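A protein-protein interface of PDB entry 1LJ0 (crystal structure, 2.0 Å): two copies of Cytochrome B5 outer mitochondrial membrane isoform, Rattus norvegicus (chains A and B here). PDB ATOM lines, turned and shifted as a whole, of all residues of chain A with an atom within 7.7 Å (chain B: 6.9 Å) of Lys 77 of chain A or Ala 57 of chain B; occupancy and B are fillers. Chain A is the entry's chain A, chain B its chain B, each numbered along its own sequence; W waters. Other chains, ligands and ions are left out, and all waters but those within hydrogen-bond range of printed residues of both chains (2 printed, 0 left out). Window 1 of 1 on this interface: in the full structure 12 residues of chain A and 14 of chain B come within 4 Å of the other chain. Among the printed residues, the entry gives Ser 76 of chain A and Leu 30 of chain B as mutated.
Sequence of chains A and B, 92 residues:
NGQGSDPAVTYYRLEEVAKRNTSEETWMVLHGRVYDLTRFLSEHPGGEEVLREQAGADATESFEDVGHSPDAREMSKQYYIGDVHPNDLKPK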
ATOM      1  N   ARG A  33       2.379 -12.005  30.881  1.00  0.00           N
ATOM      2  CA  ARG A  33       1.047 -11.393  30.685  1.00  0.00           C
ATOM      3  C   ARG A  33       0.202 -11.637  31.902  1.00  0.00           C
ATOM      4  O   ARG A  33       0.363 -12.667  32.608  1.00  0.00           O
ATOM      5  CB  ARG A  33       0.335 -11.939  29.425  1.00  0.00           C
ATOM      6  CG  ARG A  33       1.069 -11.516  28.162  1.00  0.00           C
ATOM      7  CD  ARG A  33       0.390 -12.009  26.879  1.00  0.00           C
ATOM      8  NE  ARG A  33       0.947 -11.309  25.732  1.00  0.00           N
ATOM      9  CZ  ARG A  33       0.373 -11.271  24.528  1.00  0.00           C
ATOM     10  NH1 ARG A  33      -0.775 -11.920  24.303  1.00  0.00           N
ATOM     11  NH2 ARG A  33       0.922 -10.534  23.574  1.00  0.00           N
ATOM     12  N   VAL A  34      -0.693 -10.703  32.149  1.00  0.00           N
ATOM     13  CA  VAL A  34      -1.588 -10.755  33.308  1.00  0.00           C
ATOM     14  C   VAL A  34      -2.968 -11.251  32.901  1.00  0.00           C
ATOM     15  O   VAL A  34      -3.525 -10.839  31.881  1.00  0.00           O
ATOM     16  CB  VAL A  34      -1.715  -9.354  33.965  1.00  0.00           C
ATOM     17  CG1 VAL A  34      -2.683  -9.385  35.171  1.00  0.00           C
ATOM     18  CG2 VAL A  34      -0.349  -8.885  34.406  1.00  0.00           C
ATOM     19  N   TYR A  35      -3.516 -12.135  33.724  1.00  0.00           N
ATOM     20  CA  TYR A  35      -4.805 -12.730  33.450  1.00  0.00           C
ATOM     21  C   TYR A  35      -5.710 -12.558  34.621  1.00  0.00           C
ATOM     22  O   TYR A  35      -5.277 -12.774  35.753  1.00  0.00           O
ATOM     23  CB  TYR A  35      -4.680 -14.213  33.185  1.00  0.00           C
ATOM     24  CG  TYR A  35      -3.935 -14.513  31.928  1.00  0.00           C
ATOM     25  CD1 TYR A  35      -2.528 -14.522  31.920  1.00  0.00           C
ATOM     26  CD2 TYR A  35      -4.619 -14.682  30.715  1.00  0.00           C
ATOM     27  CE1 TYR A  35      -1.819 -14.661  30.745  1.00  0.00           C
ATOM     28  CE2 TYR A  35      -3.929 -14.845  29.522  1.00  0.00           C
ATOM     29  CZ  TYR A  35      -2.524 -14.823  29.534  1.00  0.00           C
ATOM     30  OH  TYR A  35      -1.818 -14.943  28.355  1.00  0.00           O
ATOM     31  N   PRO A  70      -3.516 -27.506  24.159  1.00  0.00           N
ATOM     32  CA  PRO A  70      -3.696 -26.372  23.251  1.00  0.00           C
ATOM     33  C   PRO A  70      -5.028 -25.700  23.636  1.00  0.00           C
ATOM     34  O   PRO A  70      -5.164 -24.461  23.621  1.00  0.00           O
ATOM     35  CB  PRO A  70      -3.822 -27.045  21.878  1.00  0.00           C
ATOM     36  CG  PRO A  70      -3.051 -28.321  22.046  1.00  0.00           C
ATOM     37  CD  PRO A  70      -3.224 -28.765  23.440  1.00  0.00           C
ATOM     38  N   ASP A  71      -6.029 -26.518  24.002  1.00  0.00           N
ATOM     39  CA  ASP A  71      -7.338 -25.915  24.325  1.00  0.00           C
ATOM     40  C   ASP A  71      -7.295 -25.102  25.621  1.00  0.00           C
ATOM     41  O   ASP A  71      -7.984 -24.105  25.754  1.00  0.00           O
ATOM     42  CB  ASP A  71      -8.482 -26.974  24.364  1.00  0.00           C
ATOM     43  CG  ASP A  71      -8.775 -27.578  22.968  1.00  0.00           C
ATOM     44  OD1 ASP A  71      -9.004 -26.804  21.998  1.00  0.00           O
ATOM     45  OD2 ASP A  71      -8.758 -28.819  22.828  1.00  0.00           O
ATOM     46  N   ALA A  72      -6.441 -25.504  26.546  1.00  0.00           N
ATOM     47  CA  ALA A  72      -6.303 -24.797  27.808  1.00  0.00           C
ATOM     48  C   ALA A  72      -5.651 -23.443  27.505  1.00  0.00           C
ATOM     49  O   ALA A  72      -6.058 -22.392  28.010  1.00  0.00           O
ATOM     50  CB  ALA A  72      -5.458 -25.636  28.797  1.00  0.00           C
ATOM     51  N   ARG A  73      -4.661 -23.460  26.638  1.00  0.00           N
ATOM     52  CA  ARG A  73      -4.028 -22.213  26.248  1.00  0.00           C
ATOM     53  C   ARG A  73      -5.023 -21.277  25.537  1.00  0.00           C
ATOM     54  O   ARG A  73      -5.060 -20.087  25.809  1.00  0.00           O
ATOM     55  CB  ARG A  73      -2.831 -22.487  25.330  1.00  0.00           C
ATOM     56  CG  ARG A  73      -1.747 -23.224  26.042  1.00  0.00           C
ATOM     57  CD  ARG A  73      -0.673 -23.621  25.038  1.00  0.00           C
ATOM     58  NE  ARG A  73       0.208 -24.641  25.572  1.00  0.00           N
ATOM     59  CZ  ARG A  73       1.226 -24.437  26.414  1.00  0.00           C
ATOM     60  NH1 ARG A  73       1.506 -23.229  26.851  1.00  0.00           N
ATOM     61  NH2 ARG A  73       2.019 -25.462  26.762  1.00  0.00           N
ATOM     62  N   GLU A  74      -5.827 -21.813  24.633  1.00  0.00           N
ATOM     63  CA  GLU A  74      -6.804 -20.977  23.914  1.00  0.00           C
ATOM     64  C   GLU A  74      -7.783 -20.312  24.906  1.00  0.00           C
ATOM     65  O   GLU A  74      -8.158 -19.122  24.792  1.00  0.00           O
ATOM     66  CB  GLU A  74      -7.589 -21.865  22.919  1.00  0.00           C
ATOM     67  CG  GLU A  74      -8.639 -21.105  22.168  1.00  0.00           C
ATOM     68  CD  GLU A  74      -8.064 -19.958  21.373  1.00  0.00           C
ATOM     69  OE1 GLU A  74      -6.873 -20.023  20.993  1.00  0.00           O
ATOM     70  OE2 GLU A  74      -8.808 -18.997  21.113  1.00  0.00           O
ATOM     71  N   MET A  75      -8.172 -21.105  25.893  1.00  0.00           N
ATOM     72  CA  MET A  75      -9.106 -20.711  26.947  1.00  0.00           C
ATOM     73  C   MET A  75      -8.560 -19.550  27.808  1.00  0.00           C
ATOM     74  O   MET A  75      -9.297 -18.696  28.272  1.00  0.00           O
ATOM     75  CB  MET A  75      -9.394 -21.956  27.797  1.00  0.00           C
ATOM     76  CG  MET A  75     -10.491 -21.839  28.811  1.00  0.00           C
ATOM     77  SD  MET A  75     -10.711 -23.353  29.841  1.00  0.00           S
ATOM     78  CE  MET A  75     -11.191 -24.600  28.620  1.00  0.00           C
ATOM     79  N   SER A  76      -7.258 -19.495  27.981  1.00  0.00           N
ATOM     80  CA  SER A  76      -6.683 -18.424  28.791  1.00  0.00           C
ATOM     81  C   SER A  76      -6.811 -17.038  28.153  1.00  0.00           C
ATOM     82  O   SER A  76      -6.858 -16.028  28.858  1.00  0.00           O
ATOM     83  CB  SER A  76      -5.224 -18.689  29.024  1.00  0.00           C
ATOM     84  OG  SER A  76      -4.504 -18.446  27.830  1.00  0.00           O
ATOM     85  N   LYS A  77      -6.886 -17.005  26.826  1.00  0.00           N
ATOM     86  CA  LYS A  77      -6.919 -15.725  26.111  1.00  0.00           C
ATOM     87  C   LYS A  77      -8.034 -14.786  26.559  1.00  0.00           C
ATOM     88  O   LYS A  77      -7.827 -13.598  26.734  1.00  0.00           O
ATOM     89  CB  LYS A  77      -7.014 -15.946  24.592  1.00  0.00           C
ATOM     90  CG  LYS A  77      -5.841 -16.666  23.964  1.00  0.00           C
ATOM     91  CD  LYS A  77      -6.213 -16.777  22.440  1.00  0.00           C
ATOM     92  CE  LYS A  77      -5.135 -17.400  21.586  1.00  0.00           C
ATOM     93  NZ  LYS A  77      -5.732 -17.727  20.200  1.00  0.00           N
ATOM     94  N   GLN A  78      -9.210 -15.323  26.809  1.00  0.00           N
ATOM     95  CA  GLN A  78     -10.289 -14.443  27.210  1.00  0.00           C
ATOM     96  C   GLN A  78     -10.044 -13.678  28.538  1.00  0.00           C
ATOM     97  O   GLN A  78     -10.742 -12.697  28.829  1.00  0.00           O
ATOM     98  CB  GLN A  78     -11.572 -15.257  27.348  1.00  0.00           C
ATOM     99  CG  GLN A  78     -11.385 -16.380  28.309  1.00  0.00           C
ATOM    100  CD  GLN A  78     -12.560 -17.322  28.300  1.00  0.00           C
ATOM    101  OE1 GLN A  78     -13.691 -16.873  28.442  1.00  0.00           O
ATOM    102  NE2 GLN A  78     -12.303 -18.639  28.138  1.00  0.00           N
ATOM    103  N   TYR A  79      -9.099 -14.145  29.344  1.00  0.00           N
ATOM    104  CA  TYR A  79      -8.838 -13.505  30.646  1.00  0.00           C
ATOM    105  C   TYR A  79      -7.653 -12.543  30.611  1.00  0.00           C
ATOM    106  O   TYR A  79      -7.339 -11.894  31.602  1.00  0.00           O
ATOM    107  CB  TYR A  79      -8.604 -14.607  31.688  1.00  0.00           C
ATOM    108  CG  TYR A  79      -9.783 -15.587  31.761  1.00  0.00           C
ATOM    109  CD1 TYR A  79     -11.033 -15.157  32.214  1.00  0.00           C
ATOM    110  CD2 TYR A  79      -9.671 -16.906  31.319  1.00  0.00           C
ATOM    111  CE1 TYR A  79     -12.163 -16.030  32.220  1.00  0.00           C
ATOM    112  CE2 TYR A  79     -10.805 -17.792  31.313  1.00  0.00           C
ATOM    113  CZ  TYR A  79     -12.030 -17.326  31.769  1.00  0.00           C
ATOM    114  OH  TYR A  79     -13.124 -18.147  31.780  1.00  0.00           O
ATOM    115  N   TYR A  80      -6.991 -12.463  29.463  1.00  0.00           N
ATOM    116  CA  TYR A  80      -5.828 -11.591  29.337  1.00  0.00           C
ATOM    117  C   TYR A  80      -6.245 -10.115  29.541  1.00  0.00           C
ATOM    118  O   TYR A  80      -7.132  -9.611  28.867  1.00  0.00           O
ATOM    119  CB  TYR A  80      -5.209 -11.836  27.962  1.00  0.00           C
ATOM    120  CG  TYR A  80      -4.161 -10.824  27.458  1.00  0.00           C
ATOM    121  CD1 TYR A  80      -3.079 -10.437  28.242  1.00  0.00           C
ATOM    122  CD2 TYR A  80      -4.230 -10.335  26.150  1.00  0.00           C
ATOM    123  CE1 TYR A  80      -2.069  -9.575  27.724  1.00  0.00           C
ATOM    124  CE2 TYR A  80      -3.248  -9.495  25.630  1.00  0.00           C
ATOM    125  CZ  TYR A  80      -2.170  -9.111  26.409  1.00  0.00           C
ATOM    126  OH  TYR A  80      -1.243  -8.219  25.864  1.00  0.00           O
ATOM    127  N   ILE A  81      -5.640  -9.446  30.518  1.00  0.00           N
ATOM    128  CA  ILE A  81      -5.963  -8.043  30.752  1.00  0.00           C
ATOM    129  C   ILE A  81      -4.786  -7.150  30.485  1.00  0.00           C
ATOM    130  O   ILE A  81      -4.937  -5.955  30.326  1.00  0.00           O
ATOM    131  CB  ILE A  81      -6.460  -7.755  32.166  1.00  0.00           C
ATOM    132  CG1 ILE A  81      -5.469  -8.298  33.221  1.00  0.00           C
ATOM    133  CG2 ILE A  81      -7.907  -8.241  32.283  1.00  0.00           C
ATOM    134  CD1 ILE A  81      -5.787  -7.823  34.645  1.00  0.00           C
ATOM    135  N   LEU B  14       4.339 -25.955  22.240  1.00  0.00           N
ATOM    136  CA  LEU B  14       3.591 -24.694  22.425  1.00  0.00           C
ATOM    137  C   LEU B  14       4.121 -23.848  23.574  1.00  0.00           C
ATOM    138  O   LEU B  14       3.869 -22.634  23.642  1.00  0.00           O
ATOM    139  CB  LEU B  14       2.110 -24.969  22.645  1.00  0.00           C
ATOM    140  CG  LEU B  14       1.330 -25.453  21.403  1.00  0.00           C
ATOM    141  CD1 LEU B  14      -0.110 -25.760  21.789  1.00  0.00           C
ATOM    142  CD2 LEU B  14       1.379 -24.384  20.283  1.00  0.00           C
ATOM    143  N   VAL B  17       6.656 -21.647  22.022  1.00  0.00           N
ATOM    144  CA  VAL B  17       6.007 -20.606  21.240  1.00  0.00           C
ATOM    145  C   VAL B  17       5.484 -19.512  22.200  1.00  0.00           C
ATOM    146  O   VAL B  17       5.666 -18.315  21.952  1.00  0.00           O
ATOM    147  CB  VAL B  17       4.824 -21.183  20.393  1.00  0.00           C
ATOM    148  CG1 VAL B  17       4.097 -20.064  19.731  1.00  0.00           C
ATOM    149  CG2 VAL B  17       5.356 -22.199  19.325  1.00  0.00           C
ATOM    150  N   ALA B  18       4.865 -19.940  23.307  1.00  0.00           N
ATOM    151  CA  ALA B  18       4.302 -19.005  24.317  1.00  0.00           C
ATOM    152  C   ALA B  18       5.292 -17.983  24.874  1.00  0.00           C
ATOM    153  O   ALA B  18       4.878 -16.896  25.305  1.00  0.00           O
ATOM    154  CB  ALA B  18       3.672 -19.780  25.465  1.00  0.00           C
ATOM    155  N   ARG B  20       7.665 -16.469  23.127  1.00  0.00           N
ATOM    156  CA  ARG B  20       7.859 -15.462  22.113  1.00  0.00           C
ATOM    157  C   ARG B  20       6.619 -14.607  21.905  1.00  0.00           C
ATOM    158  O   ARG B  20       5.944 -14.719  20.864  1.00  0.00           O
ATOM    159  CB  ARG B  20       8.258 -16.105  20.789  1.00  0.00           C
ATOM    160  CG  ARG B  20       9.737 -16.478  20.723  1.00  0.00           C
ATOM    161  CD  ARG B  20      10.035 -17.660  21.605  1.00  0.00           C
ATOM    162  NE  ARG B  20      11.405 -18.128  21.376  1.00  0.00           N
ATOM    163  CZ  ARG B  20      11.892 -19.322  21.736  1.00  0.00           C
ATOM    164  NH1 ARG B  20      11.138 -20.236  22.366  1.00  0.00           N
ATOM    165  NH2 ARG B  20      13.157 -19.603  21.442  1.00  0.00           N
ATOM    166  N   ASN B  21       6.363 -13.736  22.875  1.00  0.00           N
ATOM    167  CA  ASN B  21       5.192 -12.870  22.796  1.00  0.00           C
ATOM    168  C   ASN B  21       5.548 -11.411  23.018  1.00  0.00           C
ATOM    169  O   ASN B  21       4.770 -10.671  23.567  1.00  0.00           O
ATOM    170  CB  ASN B  21       4.147 -13.336  23.807  1.00  0.00           C
ATOM    171  CG  ASN B  21       4.658 -13.260  25.252  1.00  0.00           C
ATOM    172  OD1 ASN B  21       5.765 -12.797  25.493  1.00  0.00           O
ATOM    173  ND2 ASN B  21       3.846 -13.702  26.196  1.00  0.00           N
ATOM    174  N   TRP B  27       6.302 -15.127  17.867  1.00  0.00           N
ATOM    175  CA  TRP B  27       6.014 -16.319  17.100  1.00  0.00           C
ATOM    176  C   TRP B  27       4.546 -16.543  17.212  1.00  0.00           C
ATOM    177  O   TRP B  27       3.910 -16.071  18.151  1.00  0.00           O
ATOM    178  CB  TRP B  27       6.716 -17.546  17.661  1.00  0.00           C
ATOM    179  CG  TRP B  27       8.185 -17.542  17.491  1.00  0.00           C
ATOM    180  CD1 TRP B  27       8.958 -16.535  16.994  1.00  0.00           C
ATOM    181  CD2 TRP B  27       9.061 -18.608  17.813  1.00  0.00           C
ATOM    182  NE1 TRP B  27      10.282 -16.911  16.987  1.00  0.00           N
ATOM    183  CE2 TRP B  27      10.372 -18.186  17.491  1.00  0.00           C
ATOM    184  CE3 TRP B  27       8.872 -19.899  18.358  1.00  0.00           C
ATOM    185  CZ2 TRP B  27      11.506 -19.018  17.687  1.00  0.00           C
ATOM    186  CZ3 TRP B  27      10.018 -20.737  18.558  1.00  0.00           C
ATOM    187  CH2 TRP B  27      11.302 -20.280  18.219  1.00  0.00           C
ATOM    188  N   MET B  28       4.011 -17.316  16.279  1.00  0.00           N
ATOM    189  CA  MET B  28       2.601 -17.585  16.266  1.00  0.00           C
ATOM    190  C   MET B  28       2.316 -18.899  15.559  1.00  0.00           C
ATOM    191  O   MET B  28       3.014 -19.278  14.619  1.00  0.00           O
ATOM    192  CB  MET B  28       1.926 -16.430  15.550  1.00  0.00           C
ATOM    193  CG  MET B  28       0.495 -16.249  15.839  1.00  0.00           C
ATOM    194  SD  MET B  28      -0.012 -14.644  15.051  1.00  0.00           S
ATOM    195  CE  MET B  28       0.838 -13.506  16.161  1.00  0.00           C
ATOM    196  N   VAL B  29       1.285 -19.602  16.010  1.00  0.00           N
ATOM    197  CA  VAL B  29       0.927 -20.848  15.357  1.00  0.00           C
ATOM    198  C   VAL B  29      -0.300 -20.681  14.432  1.00  0.00           C
ATOM    199  O   VAL B  29      -1.288 -19.979  14.737  1.00  0.00           O
ATOM    200  CB  VAL B  29       0.646 -21.977  16.395  1.00  0.00           C
ATOM    201  CG1 VAL B  29      -0.074 -23.191  15.715  1.00  0.00           C
ATOM    202  CG2 VAL B  29       1.952 -22.470  16.959  1.00  0.00           C
ATOM    203  N   LEU B  30      -0.184 -21.279  13.255  1.00  0.00           N
ATOM    204  CA  LEU B  30      -1.284 -21.288  12.315  1.00  0.00           C
ATOM    205  C   LEU B  30      -1.338 -22.728  11.791  1.00  0.00           C
ATOM    206  O   LEU B  30      -0.353 -23.248  11.231  1.00  0.00           O
ATOM    207  CB  LEU B  30      -1.046 -20.282  11.189  1.00  0.00           C
ATOM    208  CG  LEU B  30      -1.144 -18.795  11.562  1.00  0.00           C
ATOM    209  CD1 LEU B  30      -0.785 -17.954  10.373  1.00  0.00           C
ATOM    210  CD2 LEU B  30      -2.568 -18.452  11.999  1.00  0.00           C
ATOM    211  N   GLU B  53      -1.754  -8.904  19.985  1.00  0.00           N
ATOM    212  CA  GLU B  53      -2.738  -9.505  20.880  1.00  0.00           C
ATOM    213  C   GLU B  53      -2.630 -11.040  21.012  1.00  0.00           C
ATOM    214  O   GLU B  53      -2.787 -11.581  22.098  1.00  0.00           O
ATOM    215  CB  GLU B  53      -4.102  -9.138  20.402  1.00  0.00           C
ATOM    216  CG  GLU B  53      -5.207  -9.524  21.300  1.00  0.00           C
ATOM    217  CD  GLU B  53      -6.502  -9.445  20.522  1.00  0.00           C
ATOM    218  OE1 GLU B  53      -6.722  -8.398  19.868  1.00  0.00           O
ATOM    219  OE2 GLU B  53      -7.266 -10.438  20.539  1.00  0.00           O
ATOM    220  N   GLN B  54      -2.332 -11.720  19.915  1.00  0.00           N
ATOM    221  CA  GLN B  54      -2.185 -13.153  19.944  1.00  0.00           C
ATOM    222  C   GLN B  54      -0.742 -13.649  19.787  1.00  0.00           C
ATOM    223  O   GLN B  54      -0.505 -14.770  19.354  1.00  0.00           O
ATOM    224  CB  GLN B  54      -3.084 -13.760  18.903  1.00  0.00           C
ATOM    225  CG  GLN B  54      -4.501 -13.704  19.427  1.00  0.00           C
ATOM    226  CD  GLN B  54      -5.433 -14.459  18.569  1.00  0.00           C
ATOM    227  OE1 GLN B  54      -5.421 -15.693  18.563  1.00  0.00           O
ATOM    228  NE2 GLN B  54      -6.259 -13.741  17.829  1.00  0.00           N
ATOM    229  N   ALA B  55       0.210 -12.803  20.174  1.00  0.00           N
ATOM    230  CA  ALA B  55       1.625 -13.128  20.090  1.00  0.00           C
ATOM    231  C   ALA B  55       1.928 -14.347  20.974  1.00  0.00           C
ATOM    232  O   ALA B  55       1.465 -14.409  22.097  1.00  0.00           O
ATOM    233  CB  ALA B  55       2.496 -11.872  20.523  1.00  0.00           C
ATOM    234  N   GLY B  56       2.710 -15.296  20.458  1.00  0.00           N
ATOM    235  CA  GLY B  56       3.050 -16.506  21.208  1.00  0.00           C
ATOM    236  C   GLY B  56       1.912 -17.514  21.255  1.00  0.00           C
ATOM    237  O   GLY B  56       2.018 -18.506  21.907  1.00  0.00           O
ATOM    238  N   ALA B  57       0.831 -17.272  20.533  1.00  0.00           N
ATOM    239  CA  ALA B  57      -0.320 -18.163  20.585  1.00  0.00           C
ATOM    240  C   ALA B  57      -0.714 -18.768  19.254  1.00  0.00           C
ATOM    241  O   ALA B  57      -0.156 -18.459  18.221  1.00  0.00           O
ATOM    242  CB  ALA B  57      -1.496 -17.405  21.141  1.00  0.00           C
ATOM    243  N   ASP B  58      -1.706 -19.644  19.313  1.00  0.00           N
ATOM    244  CA  ASP B  58      -2.260 -20.257  18.134  1.00  0.00           C
ATOM    245  C   ASP B  58      -3.391 -19.328  17.682  1.00  0.00           C
ATOM    246  O   ASP B  58      -4.464 -19.285  18.290  1.00  0.00           O
ATOM    247  CB  ASP B  58      -2.801 -21.650  18.469  1.00  0.00           C
ATOM    248  CG  ASP B  58      -3.336 -22.386  17.232  1.00  0.00           C
ATOM    249  OD1 ASP B  58      -3.810 -21.713  16.283  1.00  0.00           O
ATOM    250  OD2 ASP B  58      -3.284 -23.638  17.230  1.00  0.00           O
ATOM    251  N   ALA B  59      -3.168 -18.590  16.605  1.00  0.00           N
ATOM    252  CA  ALA B  59      -4.199 -17.665  16.100  1.00  0.00           C
ATOM    253  C   ALA B  59      -4.909 -18.214  14.834  1.00  0.00           C
ATOM    254  O   ALA B  59      -5.433 -17.470  14.003  1.00  0.00           O
ATOM    255  CB  ALA B  59      -3.550 -16.299  15.807  1.00  0.00           C
ATOM    256  N   THR B  60      -4.933 -19.521  14.689  1.00  0.00           N
ATOM    257  CA  THR B  60      -5.588 -20.115  13.520  1.00  0.00           C
ATOM    258  C   THR B  60      -7.030 -19.644  13.330  1.00  0.00           C
ATOM    259  O   THR B  60      -7.416 -19.179  12.250  1.00  0.00           O
ATOM    260  CB  THR B  60      -5.612 -21.628  13.620  1.00  0.00           C
ATOM    261  OG1 THR B  60      -4.270 -22.099  13.706  1.00  0.00           O
ATOM    262  CG2 THR B  60      -6.332 -22.254  12.370  1.00  0.00           C
ATOM    263  N   GLU B  61      -7.829 -19.766  14.379  1.00  0.00           N
ATOM    264  CA  GLU B  61      -9.211 -19.367  14.269  1.00  0.00           C
ATOM    265  C   GLU B  61      -9.368 -17.901  13.851  1.00  0.00           C
ATOM    266  O   GLU B  61     -10.130 -17.599  12.919  1.00  0.00           O
ATOM    267  CB  GLU B  61      -9.952 -19.694  15.581  1.00  0.00           C
ATOM    268  CG  GLU B  61     -10.148 -21.212  15.776  1.00  0.00           C
ATOM    269  CD  GLU B  61     -10.862 -21.882  14.604  1.00  0.00           C
ATOM    270  OE1 GLU B  61     -11.977 -21.422  14.228  1.00  0.00           O
ATOM    271  OE2 GLU B  61     -10.320 -22.876  14.051  1.00  0.00           O
ATOM    272  N   SER B  62      -8.654 -16.984  14.497  1.00  0.00           N
ATOM    273  CA  SER B  62      -8.758 -15.585  14.082  1.00  0.00           C
ATOM    274  C   SER B  62      -8.317 -15.397  12.638  1.00  0.00           C
ATOM    275  O   SER B  62      -8.955 -14.644  11.885  1.00  0.00           O
ATOM    276  CB  SER B  62      -7.934 -14.650  14.993  1.00  0.00           C
ATOM    277  OG  SER B  62      -8.492 -14.626  16.284  1.00  0.00           O
HETATM  278  O   HOH W   1       3.317  -9.826  25.925  1.00  0.00           O
HETATM  279  O   HOH W   2       3.674 -27.412  25.197  1.00  0.00           O
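No position is printed for both chains.
Lys 77 of chain A touches three residues of chain B. Ala 57 of chain B touches just one residue of chain A: Lys 77 (3.7 Å). Gly 56 of chain B touches none of the printed residues of chain A. Of the printed residues of chain B, Pro 70 of chain A touches Leu 14 (3.9 Å). Of the printed residues of chain A, Asp 58 of chain B touches Glu 74 and Lys 77. Printed residues of chain B within 4 Å of Arg 33 of chain A: Asn 21, Glu 53 and Ala 55. Of the printed residues of chain B, Glu 74 of chain A touches Asp 58. Tyr 80 of chain A touches none of the printed residues of chain B.
NE2 of Gln 54 of chain B lies within hydrogen-bond range of OG of Ser 62 of chain B, at 2.9 Å. The side-chain amino group of Lys 77 of chain A lies within salt-bridge range of the side-chain carboxylate of Glu 74 of chain A. The backbone carbonyl oxygen of Ala 18 of chain B is in hydrogen-bond range of the side-chain amide nitrogen of Asn 21 of chain B (3.5 Å). N of Val 29 of chain B sits at hydrogen-bond distance from O of Ala 57 of chain B, 2.9 Å away. The backbone carbonyl oxygen (O) of Arg 73 of chain A is in hydrogen-bond range of the side-chain hydroxyl (OG) of Ser 76 of chain A. OD1 of Asp 58 of chain B lies within hydrogen-bond range of OG1 of Thr 60 of chain B (2.6 Å).
NZ of Lys 77 of chain A lies within hydrogen-bond range of O of Asp 58 of chain B (2.8 Å). The side-chain amino group (NZ) of Lys 77 of chain A sits at hydrogen-bond distance from the side-chain amide oxygen (OE1) of Gln 54 of chain B, at 2.6 Å. NH1 of Arg 33 of chain A is in hydrogen-bond range of O of Glu 53 of chain B (3.0 Å).
Arg 33 of chain A touches Asn 21 of chain B. Ala 55 of chain B touches Arg 33 of chain A. Pro 70 of chain A touches Leu 14 of chain B. NE of Arg 73 of chain A touches CB of Leu 14 of chain B (3.5 Å). Glu 74 of chain A touches Asp 58 of chain B (OE1 to O, 3.7 Å). Lys 77 of chain A touches Ala 57 of chain B.
Water W1 lies within hydrogen-bond range of NE of Arg 33 of chain A (2.8 Å) and O of Asn 21 of chain B (2.9 Å). Water W2 bridges the guanidinium group of Arg 73 of chain A (3.0 Å) and the backbone NH of Leu 14 of chain B (3.4 Å).
Printed residues of chain A that touch a printed residue of chain B: Arg 33, Pro 70, Arg 73, Glu 74 and Lys 77. Hydrophobic or aromatic side chains of chain A that line the printed part of chain B: Pro 70. Of the 19 printed residues of chain B, 7 touch a printed residue of chain A. Hydrophobic or aromatic side chains of chain B that line the printed part of chain A: Leu 14, Ala 55 and Ala 57. Among the printed residues, 9 pairs touch across the chains. Among the printed residues, no Asp or Glu carboxylate lies within 4 Å of a Lys or Arg side-chain nitrogen of the other chain.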
